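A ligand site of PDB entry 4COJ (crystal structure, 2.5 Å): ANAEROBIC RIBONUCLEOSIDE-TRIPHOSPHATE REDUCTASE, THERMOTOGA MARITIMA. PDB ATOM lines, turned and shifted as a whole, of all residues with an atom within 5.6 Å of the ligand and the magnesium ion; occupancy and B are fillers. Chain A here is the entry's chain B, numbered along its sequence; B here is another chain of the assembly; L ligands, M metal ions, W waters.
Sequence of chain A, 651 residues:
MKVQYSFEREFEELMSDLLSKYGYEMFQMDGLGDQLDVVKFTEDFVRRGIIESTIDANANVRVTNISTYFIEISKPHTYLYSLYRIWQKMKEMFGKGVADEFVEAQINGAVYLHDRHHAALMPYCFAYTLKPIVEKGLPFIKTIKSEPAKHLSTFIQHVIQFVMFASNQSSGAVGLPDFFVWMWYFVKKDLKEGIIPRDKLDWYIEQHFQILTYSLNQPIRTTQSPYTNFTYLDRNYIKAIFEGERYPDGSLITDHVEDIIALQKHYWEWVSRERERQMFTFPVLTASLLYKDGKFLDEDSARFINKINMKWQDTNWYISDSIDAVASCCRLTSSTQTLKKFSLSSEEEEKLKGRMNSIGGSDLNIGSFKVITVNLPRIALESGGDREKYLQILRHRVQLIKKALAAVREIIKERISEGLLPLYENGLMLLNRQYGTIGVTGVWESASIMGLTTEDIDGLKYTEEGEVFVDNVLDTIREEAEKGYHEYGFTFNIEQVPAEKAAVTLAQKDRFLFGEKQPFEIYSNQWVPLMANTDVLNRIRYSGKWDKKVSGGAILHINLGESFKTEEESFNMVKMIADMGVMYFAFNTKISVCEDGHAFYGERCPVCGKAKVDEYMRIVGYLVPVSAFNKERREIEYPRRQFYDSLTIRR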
ATOM      1  N   LEU A 138     -31.744 -28.228  33.821  1.00  0.00           N
ATOM      2  CA  LEU A 138     -33.202 -28.271  33.933  1.00  0.00           C
ATOM      3  C   LEU A 138     -33.757 -29.547  33.292  1.00  0.00           C
ATOM      4  O   LEU A 138     -34.201 -29.535  32.149  1.00  0.00           O
ATOM      5  CB  LEU A 138     -33.835 -27.042  33.288  1.00  0.00           C
ATOM      6  CG  LEU A 138     -33.261 -25.687  33.722  1.00  0.00           C
ATOM      7  CD1 LEU A 138     -33.927 -24.558  32.958  1.00  0.00           C
ATOM      8  CD2 LEU A 138     -33.414 -25.479  35.204  1.00  0.00           C
ATOM      9  N   LYS A 145     -35.714 -29.793  27.730  1.00  0.00           N
ATOM     10  CA  LYS A 145     -34.725 -30.102  28.757  1.00  0.00           C
ATOM     11  C   LYS A 145     -33.392 -29.388  28.494  1.00  0.00           C
ATOM     12  O   LYS A 145     -32.878 -29.396  27.367  1.00  0.00           O
ATOM     13  CB  LYS A 145     -34.507 -31.614  28.836  1.00  0.00           C
ATOM     14  CG  LYS A 145     -35.758 -32.361  29.320  1.00  0.00           C
ATOM     15  CD  LYS A 145     -35.532 -33.861  29.391  1.00  0.00           C
ATOM     16  CE  LYS A 145     -36.718 -34.572  30.035  1.00  0.00           C
ATOM     17  NZ  LYS A 145     -37.945 -34.530  29.181  1.00  0.00           N
ATOM     18  N   SER A 146     -32.859 -28.780  29.540  1.00  0.00           N
ATOM     19  CA  SER A 146     -31.614 -28.028  29.479  1.00  0.00           C
ATOM     20  C   SER A 146     -30.496 -28.745  30.214  1.00  0.00           C
ATOM     21  O   SER A 146     -30.668 -29.168  31.366  1.00  0.00           O
ATOM     22  CB  SER A 146     -31.798 -26.635  30.074  1.00  0.00           C
ATOM     23  OG  SER A 146     -32.846 -25.922  29.439  1.00  0.00           O
ATOM     24  N   GLU A 147     -29.365 -28.892  29.550  1.00  0.00           N
ATOM     25  CA  GLU A 147     -28.169 -29.446  30.180  1.00  0.00           C
ATOM     26  C   GLU A 147     -27.666 -28.464  31.217  1.00  0.00           C
ATOM     27  O   GLU A 147     -28.087 -27.311  31.229  1.00  0.00           O
ATOM     28  CB  GLU A 147     -27.082 -29.714  29.133  1.00  0.00           C
ATOM     29  CG  GLU A 147     -27.506 -30.624  27.988  1.00  0.00           C
ATOM     30  CD  GLU A 147     -27.482 -32.095  28.358  1.00  0.00           C
ATOM     31  OE1 GLU A 147     -27.561 -32.422  29.566  1.00  0.00           O
ATOM     32  OE2 GLU A 147     -27.380 -32.938  27.431  1.00  0.00           O
ATOM     33  N   PRO A 148     -26.778 -28.920  32.115  1.00  0.00           N
ATOM     34  CA  PRO A 148     -26.145 -27.998  33.064  1.00  0.00           C
ATOM     35  C   PRO A 148     -25.480 -26.818  32.354  1.00  0.00           C
ATOM     36  O   PRO A 148     -24.839 -27.012  31.316  1.00  0.00           O
ATOM     37  CB  PRO A 148     -25.106 -28.879  33.763  1.00  0.00           C
ATOM     38  CG  PRO A 148     -25.692 -30.250  33.689  1.00  0.00           C
ATOM     39  CD  PRO A 148     -26.425 -30.329  32.386  1.00  0.00           C
ATOM     40  N   ALA A 149     -25.670 -25.623  32.891  1.00  0.00           N
ATOM     41  CA  ALA A 149     -25.200 -24.399  32.239  1.00  0.00           C
ATOM     42  C   ALA A 149     -23.685 -24.393  32.072  1.00  0.00           C
ATOM     43  O   ALA A 149     -22.963 -25.065  32.820  1.00  0.00           O
ATOM     44  CB  ALA A 149     -25.627 -23.182  33.039  1.00  0.00           C
ATOM     45  N   LYS A 150     -23.220 -23.641  31.079  1.00  0.00           N
ATOM     46  CA  LYS A 150     -21.789 -23.521  30.795  1.00  0.00           C
ATOM     47  C   LYS A 150     -21.340 -22.070  30.734  1.00  0.00           C
ATOM     48  O   LYS A 150     -20.138 -21.792  30.630  1.00  0.00           O
ATOM     49  CB  LYS A 150     -21.456 -24.211  29.479  1.00  0.00           C
ATOM     50  CG  LYS A 150     -21.739 -25.703  29.457  1.00  0.00           C
ATOM     51  CD  LYS A 150     -21.354 -26.288  28.111  1.00  0.00           C
ATOM     52  CE  LYS A 150     -21.580 -27.786  28.056  1.00  0.00           C
ATOM     53  NZ  LYS A 150     -21.062 -28.358  26.777  1.00  0.00           N
ATOM     54  N   HIS A 151     -22.292 -21.142  30.784  1.00  0.00           N
ATOM     55  CA  HIS A 151     -21.983 -19.715  30.654  1.00  0.00           C
ATOM     56  C   HIS A 151     -22.825 -18.870  31.592  1.00  0.00           C
ATOM     57  O   HIS A 151     -23.870 -19.308  32.072  1.00  0.00           O
ATOM     58  CB  HIS A 151     -22.198 -19.252  29.214  1.00  0.00           C
ATOM     59  CG  HIS A 151     -21.554 -20.136  28.191  1.00  0.00           C
ATOM     60  ND1 HIS A 151     -20.277 -19.928  27.720  1.00  0.00           N
ATOM     61  CD2 HIS A 151     -22.016 -21.244  27.547  1.00  0.00           C
ATOM     62  CE1 HIS A 151     -19.970 -20.865  26.834  1.00  0.00           C
ATOM     63  NE2 HIS A 151     -21.012 -21.669  26.716  1.00  0.00           N
ATOM     64  N   SER A 153     -24.615 -16.279  30.867  1.00  0.00           N
ATOM     65  CA  SER A 153     -25.919 -15.979  30.275  1.00  0.00           C
ATOM     66  C   SER A 153     -26.923 -17.096  30.532  1.00  0.00           C
ATOM     67  O   SER A 153     -28.051 -16.832  30.949  1.00  0.00           O
ATOM     68  CB  SER A 153     -25.771 -15.725  28.760  1.00  0.00           C
ATOM     69  OG  SER A 153     -25.181 -16.830  28.084  1.00  0.00           O
ATOM     70  N   THR A 154     -26.513 -18.342  30.303  1.00  0.00           N
ATOM     71  CA  THR A 154     -27.378 -19.495  30.516  1.00  0.00           C
ATOM     72  C   THR A 154     -27.682 -19.727  31.992  1.00  0.00           C
ATOM     73  O   THR A 154     -28.796 -20.119  32.355  1.00  0.00           O
ATOM     74  CB  THR A 154     -26.755 -20.789  29.948  1.00  0.00           C
ATOM     75  OG1 THR A 154     -25.405 -20.523  29.529  1.00  0.00           O
ATOM     76  CG2 THR A 154     -27.558 -21.278  28.762  1.00  0.00           C
ATOM     77  N   GLN A 157     -30.255 -17.394  32.966  1.00  0.00           N
ATOM     78  CA  GLN A 157     -31.483 -17.776  32.286  1.00  0.00           C
ATOM     79  C   GLN A 157     -32.084 -19.022  32.952  1.00  0.00           C
ATOM     80  O   GLN A 157     -33.305 -19.181  32.977  1.00  0.00           O
ATOM     81  CB  GLN A 157     -31.200 -18.003  30.800  1.00  0.00           C
ATOM     82  CG  GLN A 157     -32.346 -17.734  29.853  1.00  0.00           C
ATOM     83  CD  GLN A 157     -32.850 -16.293  29.877  1.00  0.00           C
ATOM     84  OE1 GLN A 157     -32.072 -15.348  29.847  1.00  0.00           O
ATOM     85  NE2 GLN A 157     -34.182 -16.139  29.921  1.00  0.00           N
ATOM     86  N   HIS A 158     -31.225 -19.885  33.488  1.00  0.00           N
ATOM     87  CA  HIS A 158     -31.674 -21.043  34.255  1.00  0.00           C
ATOM     88  C   HIS A 158     -32.341 -20.642  35.570  1.00  0.00           C
ATOM     89  O   HIS A 158     -33.341 -21.222  35.970  1.00  0.00           O
ATOM     90  CB  HIS A 158     -30.500 -21.970  34.566  1.00  0.00           C
ATOM     91  CG  HIS A 158     -30.145 -22.893  33.445  1.00  0.00           C
ATOM     92  ND1 HIS A 158     -29.399 -24.039  33.633  1.00  0.00           N
ATOM     93  CD2 HIS A 158     -30.417 -22.848  32.122  1.00  0.00           C
ATOM     94  CE1 HIS A 158     -29.238 -24.660  32.480  1.00  0.00           C
ATOM     95  NE2 HIS A 158     -29.849 -23.959  31.545  1.00  0.00           N
ATOM     96  N   GLN A 161     -35.888 -19.577  34.723  1.00  0.00           N
ATOM     97  CA  GLN A 161     -36.806 -20.689  34.477  1.00  0.00           C
ATOM     98  C   GLN A 161     -37.141 -21.380  35.791  1.00  0.00           C
ATOM     99  O   GLN A 161     -38.243 -21.891  35.969  1.00  0.00           O
ATOM    100  CB  GLN A 161     -36.219 -21.700  33.492  1.00  0.00           C
ATOM    101  CG  GLN A 161     -35.830 -21.119  32.130  1.00  0.00           C
ATOM    102  CD  GLN A 161     -36.756 -20.016  31.656  1.00  0.00           C
ATOM    103  OE1 GLN A 161     -37.985 -20.176  31.670  1.00  0.00           O
ATOM    104  NE2 GLN A 161     -36.189 -18.893  31.244  1.00  0.00           N
ATOM    105  N   TRP B 203     -20.694 -18.501  17.671  1.00  0.00           N
ATOM    106  CA  TRP B 203     -21.153 -18.975  18.968  1.00  0.00           C
ATOM    107  C   TRP B 203     -22.074 -17.941  19.601  1.00  0.00           C
ATOM    108  O   TRP B 203     -23.071 -18.275  20.232  1.00  0.00           O
ATOM    109  CB  TRP B 203     -19.987 -19.280  19.906  1.00  0.00           C
ATOM    110  CG  TRP B 203     -20.447 -19.478  21.324  1.00  0.00           C
ATOM    111  CD1 TRP B 203     -20.784 -20.658  21.913  1.00  0.00           C
ATOM    112  CD2 TRP B 203     -20.632 -18.460  22.318  1.00  0.00           C
ATOM    113  NE1 TRP B 203     -21.166 -20.443  23.226  1.00  0.00           N
ATOM    114  CE2 TRP B 203     -21.074 -19.104  23.490  1.00  0.00           C
ATOM    115  CE3 TRP B 203     -20.456 -17.077  22.332  1.00  0.00           C
ATOM    116  CZ2 TRP B 203     -21.351 -18.399  24.662  1.00  0.00           C
ATOM    117  CZ3 TRP B 203     -20.730 -16.381  23.495  1.00  0.00           C
ATOM    118  CH2 TRP B 203     -21.174 -17.046  24.645  1.00  0.00           C
ATOM    119  N   GLU B 206     -25.417 -17.859  17.793  1.00  0.00           N
ATOM    120  CA  GLU B 206     -26.124 -19.118  18.031  1.00  0.00           C
ATOM    121  C   GLU B 206     -26.510 -19.266  19.500  1.00  0.00           C
ATOM    122  O   GLU B 206     -27.375 -20.071  19.848  1.00  0.00           O
ATOM    123  CB  GLU B 206     -25.266 -20.292  17.577  1.00  0.00           C
ATOM    124  CG  GLU B 206     -25.130 -20.360  16.049  1.00  0.00           C
ATOM    125  CD  GLU B 206     -24.152 -21.423  15.583  1.00  0.00           C
ATOM    126  OE1 GLU B 206     -24.075 -22.490  16.207  1.00  0.00           O
ATOM    127  OE2 GLU B 206     -23.455 -21.180  14.569  1.00  0.00           O
ATOM    128  N   GLN B 207     -25.874 -18.477  20.365  1.00  0.00           N
ATOM    129  CA  GLN B 207     -26.192 -18.494  21.787  1.00  0.00           C
ATOM    130  C   GLN B 207     -27.505 -17.760  22.017  1.00  0.00           C
ATOM    131  O   GLN B 207     -28.329 -18.177  22.828  1.00  0.00           O
ATOM    132  CB  GLN B 207     -25.069 -17.841  22.595  1.00  0.00           C
ATOM    133  CG  GLN B 207     -25.339 -17.755  24.087  1.00  0.00           C
ATOM    134  CD  GLN B 207     -25.204 -19.097  24.789  1.00  0.00           C
ATOM    135  OE1 GLN B 207     -25.213 -20.145  24.143  1.00  0.00           O
ATOM    136  NE2 GLN B 207     -25.055 -19.060  26.109  1.00  0.00           N
ATOM    137  N   GLN B 210     -30.194 -19.798  20.793  1.00  0.00           N
ATOM    138  CA  GLN B 210     -30.445 -20.857  21.760  1.00  0.00           C
ATOM    139  C   GLN B 210     -31.263 -20.358  22.939  1.00  0.00           C
ATOM    140  O   GLN B 210     -32.202 -21.006  23.394  1.00  0.00           O
ATOM    141  CB  GLN B 210     -29.119 -21.439  22.243  1.00  0.00           C
ATOM    142  CG  GLN B 210     -29.250 -22.785  22.922  1.00  0.00           C
ATOM    143  CD  GLN B 210     -27.929 -23.286  23.448  1.00  0.00           C
ATOM    144  OE1 GLN B 210     -27.061 -22.507  23.836  1.00  0.00           O
ATOM    145  NE2 GLN B 210     -27.762 -24.604  23.468  1.00  0.00           N
ATOM    146  N   ILE B 211     -30.904 -19.181  23.442  1.00  0.00           N
ATOM    147  CA  ILE B 211     -31.559 -18.621  24.603  1.00  0.00           C
ATOM    148  C   ILE B 211     -33.001 -18.285  24.278  1.00  0.00           C
ATOM    149  O   ILE B 211     -33.916 -18.601  25.041  1.00  0.00           O
ATOM    150  CB  ILE B 211     -30.790 -17.383  25.117  1.00  0.00           C
ATOM    151  CG1 ILE B 211     -29.538 -17.851  25.868  1.00  0.00           C
ATOM    152  CG2 ILE B 211     -31.636 -16.518  26.055  1.00  0.00           C
ATOM    153  CD1 ILE B 211     -28.507 -16.774  26.116  1.00  0.00           C
ATOM    154  N   LEU B 212     -33.224 -17.682  23.114  1.00  0.00           N
ATOM    155  CA  LEU B 212     -34.582 -17.346  22.698  1.00  0.00           C
ATOM    156  C   LEU B 212     -35.418 -18.592  22.477  1.00  0.00           C
ATOM    157  O   LEU B 212     -36.517 -18.725  23.023  1.00  0.00           O
ATOM    158  CB  LEU B 212     -34.562 -16.497  21.432  1.00  0.00           C
ATOM    159  CG  LEU B 212     -35.957 -16.117  20.903  1.00  0.00           C
ATOM    160  CD1 LEU B 212     -36.808 -15.481  21.993  1.00  0.00           C
ATOM    161  CD2 LEU B 212     -35.845 -15.184  19.732  1.00  0.00           C
ATOM    162  N   TYR B 214     -35.071 -21.749  23.468  1.00  0.00           N
ATOM    163  CA  TYR B 214     -35.355 -22.571  24.642  1.00  0.00           C
ATOM    164  C   TYR B 214     -36.371 -21.892  25.562  1.00  0.00           C
ATOM    165  O   TYR B 214     -37.171 -22.569  26.204  1.00  0.00           O
ATOM    166  CB  TYR B 214     -34.053 -22.872  25.405  1.00  0.00           C
ATOM    167  CG  TYR B 214     -33.337 -24.091  24.861  1.00  0.00           C
ATOM    168  CD1 TYR B 214     -32.645 -24.024  23.658  1.00  0.00           C
ATOM    169  CD2 TYR B 214     -33.357 -25.297  25.539  1.00  0.00           C
ATOM    170  CE1 TYR B 214     -31.992 -25.135  23.151  1.00  0.00           C
ATOM    171  CE2 TYR B 214     -32.705 -26.409  25.032  1.00  0.00           C
ATOM    172  CZ  TYR B 214     -32.030 -26.314  23.838  1.00  0.00           C
ATOM    173  OH  TYR B 214     -31.369 -27.414  23.322  1.00  0.00           O
ATOM    174  N   SER B 215     -36.360 -20.571  25.603  1.00  0.00           N
ATOM    175  CA  SER B 215     -37.343 -19.832  26.398  1.00  0.00           C
ATOM    176  C   SER B 215     -38.743 -19.947  25.809  1.00  0.00           C
ATOM    177  O   SER B 215     -39.718 -20.050  26.543  1.00  0.00           O
ATOM    178  CB  SER B 215     -36.952 -18.355  26.493  1.00  0.00           C
ATOM    179  OG  SER B 215     -36.119 -18.116  27.602  1.00  0.00           O
ATOM    180  N   GLN B 218     -40.655 -22.975  26.921  1.00  0.00           N
ATOM    181  CA  GLN B 218     -40.948 -23.100  28.352  1.00  0.00           C
ATOM    182  C   GLN B 218     -42.445 -22.988  28.546  1.00  0.00           C
ATOM    183  O   GLN B 218     -43.126 -22.327  27.752  1.00  0.00           O
ATOM    184  CB  GLN B 218     -40.223 -22.009  29.158  1.00  0.00           C
ATOM    185  CG  GLN B 218     -38.704 -22.075  29.100  1.00  0.00           C
ATOM    186  CD  GLN B 218     -38.111 -23.121  30.030  1.00  0.00           C
ATOM    187  OE1 GLN B 218     -38.555 -23.281  31.169  1.00  0.00           O
ATOM    188  NE2 GLN B 218     -37.086 -23.821  29.554  1.00  0.00           N
ATOM    189  N   GLU B 274     -29.403 -28.126  15.974  1.00  0.00           N
ATOM    190  CA  GLU B 274     -29.712 -28.183  17.396  1.00  0.00           C
ATOM    191  C   GLU B 274     -30.616 -29.347  17.775  1.00  0.00           C
ATOM    192  O   GLU B 274     -30.602 -29.806  18.919  1.00  0.00           O
ATOM    193  CB  GLU B 274     -30.367 -26.854  17.830  1.00  0.00           C
ATOM    194  CG  GLU B 274     -30.650 -26.720  19.333  1.00  0.00           C
ATOM    195  CD  GLU B 274     -29.391 -26.548  20.170  1.00  0.00           C
ATOM    196  OE1 GLU B 274     -28.279 -26.536  19.591  1.00  0.00           O
ATOM    197  OE2 GLU B 274     -29.504 -26.411  21.401  1.00  0.00           O
HETATM  198  P1  LIG L   1     -22.075 -23.776  23.995  1.00  0.00           P
HETATM  199  O1  LIG L   1     -23.038 -22.678  24.363  1.00  0.00           O
HETATM  200  O2  LIG L   1     -20.694 -23.582  24.575  1.00  0.00           O
HETATM  201  O3  LIG L   1     -22.119 -24.208  22.542  1.00  0.00           O
HETATM  202  P2  LIG L   1     -24.155 -25.064  25.324  1.00  0.00           P
HETATM  203  O4  LIG L   1     -24.577 -26.500  25.540  1.00  0.00           O
HETATM  204  O5  LIG L   1     -24.952 -24.111  24.467  1.00  0.00           O
HETATM  205  O6  LIG L   1     -22.630 -25.063  24.785  1.00  0.00           O
HETATM  206  P3  LIG L   1     -25.032 -23.403  27.448  1.00  0.00           P
HETATM  207  O7  LIG L   1     -25.205 -22.161  26.597  1.00  0.00           O
HETATM  208  O8  LIG L   1     -24.692 -23.247  28.907  1.00  0.00           O
HETATM  209  O9  LIG L   1     -23.937 -24.362  26.769  1.00  0.00           O
HETATM  210  O10 LIG L   1     -26.403 -24.247  27.379  1.00  0.00           O
HETATM  211  C1  LIG L   1     -26.613 -25.346  28.269  1.00  0.00           C
HETATM  212  C2  LIG L   1     -28.064 -25.777  28.186  1.00  0.00           C
HETATM  213  O11 LIG L   1     -28.926 -24.696  28.524  1.00  0.00           O
HETATM  214  C3  LIG L   1     -28.439 -26.241  26.781  1.00  0.00           C
HETATM  215  O12 LIG L   1     -28.995 -27.554  26.844  1.00  0.00           O
HETATM  216  C4  LIG L   1     -29.489 -25.261  26.296  1.00  0.00           C
HETATM  217  C5  LIG L   1     -30.015 -24.660  27.586  1.00  0.00           C
HETATM  218  N1  LIG L   1     -30.549 -23.286  27.411  1.00  0.00           N
HETATM  219  C6  LIG L   1     -30.063 -22.284  26.652  1.00  0.00           C
HETATM  220  N2  LIG L   1     -30.848 -21.181  26.760  1.00  0.00           N
HETATM  221  C7  LIG L   1     -31.858 -21.490  27.592  1.00  0.00           C
HETATM  222  C8  LIG L   1     -33.045 -20.799  28.138  1.00  0.00           C
HETATM  223  N3  LIG L   1     -33.312 -19.534  27.791  1.00  0.00           N
HETATM  224  N4  LIG L   1     -33.849 -21.479  28.972  1.00  0.00           N
HETATM  225  C9  LIG L   1     -33.610 -22.762  29.325  1.00  0.00           C
HETATM  226  N5  LIG L   1     -32.551 -23.443  28.864  1.00  0.00           N
HETATM  227  C10 LIG L   1     -31.664 -22.877  28.006  1.00  0.00           C
HETATM  228 MG    MG M   1     -25.102 -22.252  24.408  1.00  0.00          MG
HETATM  229  O   HOH W   1     -24.850 -21.896  21.045  1.00  0.00           O
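Within 4 Å of the magnesium ion: Gln 207 of chain B and Gln 210 of chain B. The nearest printed residue that does not touch the magnesium ion is Trp 203 of chain B (4.5 Å).
The magnesium ion is bound by an oxygen (O5) of the ligand (1.9 Å), the side-chain amide oxygen of Gln 210 of chain B (2.1 Å), an oxygen (O1) of the ligand (2.1 Å), the side-chain amide oxygen of Gln 207 of chain B (2.1 Å) and an oxygen (O7) of the ligand (2.2 Å). The magnesium ion has five donor atoms within binding distance.
The side-chain hydroxyl of Ser 215 of chain B sits close to the backbone carbonyl oxygen of Ile 211 of chain B (3.4 Å). OE2 of Glu 274 of chain B lies within hydrogen-bond range of OH of Tyr 214 of chain B. The side-chain amide oxygen of Gln 218 of chain B sits close to the side-chain amide oxygen of Gln 161. The side-chain amide nitrogen (NE2) of Gln 207 of chain B is in hydrogen-bond range of the side-chain hydroxyl (OG) of Ser 153. The backbone carbonyl oxygen (O) of Gln 157 sits close to the side-chain amide nitrogen (NE2) of Gln 161 (3.4 Å). The side-chain carboxylate (OE2) of Glu 274 of chain B lies within hydrogen-bond range of the side-chain amide nitrogen (NE2) of Gln 210 of chain B. The side-chain hydroxyl of Thr 154 is in hydrogen-bond range of the backbone carbonyl oxygen of His 151, at 3.2 Å. The backbone NH of Leu 138 sits at hydrogen-bond distance from the backbone carbonyl oxygen of Ser 146 (2.8 Å).
The indole nitrogen (NE1) of Trp 203 of chain B lies within hydrogen-bond range of an oxygen (O2) of the ligand (3.4 Å). N of Lys 150 lies within hydrogen-bond range of O8 of the ligand, at 2.7 Å. NE2 of His 151 sits at hydrogen-bond distance from O2 of the ligand, 2.9 Å away. An oxygen (O11) of the ligand sits at hydrogen-bond distance from a ring nitrogen (NE2) of His 158, at 3.2 Å. A nitrogen (N3) of the ligand sits at hydrogen-bond distance from the side-chain hydroxyl (OG) of Ser 215 of chain B, 3.2 Å away. An oxygen (O12) of the ligand sits at hydrogen-bond distance from the backbone NH of Glu 147, 3.0 Å away. An oxygen (O8) of the ligand sits at hydrogen-bond distance from the side-chain hydroxyl of Thr 154 (2.9 Å). The side-chain hydroxyl (OG) of Ser 146 sits at hydrogen-bond distance from a nitrogen (N5) of the ligand, 2.6 Å away. N3 of the ligand lies within hydrogen-bond range of O of Ile 211 of chain B (3.0 Å).
O of Pro 148 touches C1 of the ligand (3.9 Å). C of Ala 149 touches O8 of the ligand, at 3.5 Å. CG of Gln 157 touches N3 of the ligand (2.9 Å). Gln 161 touches the ligand (CG to N4, 3.7 Å). Tyr 214 of chain B touches the ligand. NE2 of Gln 218 of chain B touches C9 of the ligand, at 3.6 Å. Hydrophobic or aromatic side chains that line the ligand: His 151, His 158, Trp 203 of chain B, Ile 211 of chain B and Tyr 214 of chain B. Of the 23 residues printed, 17 come within 4 Å of the ligand.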
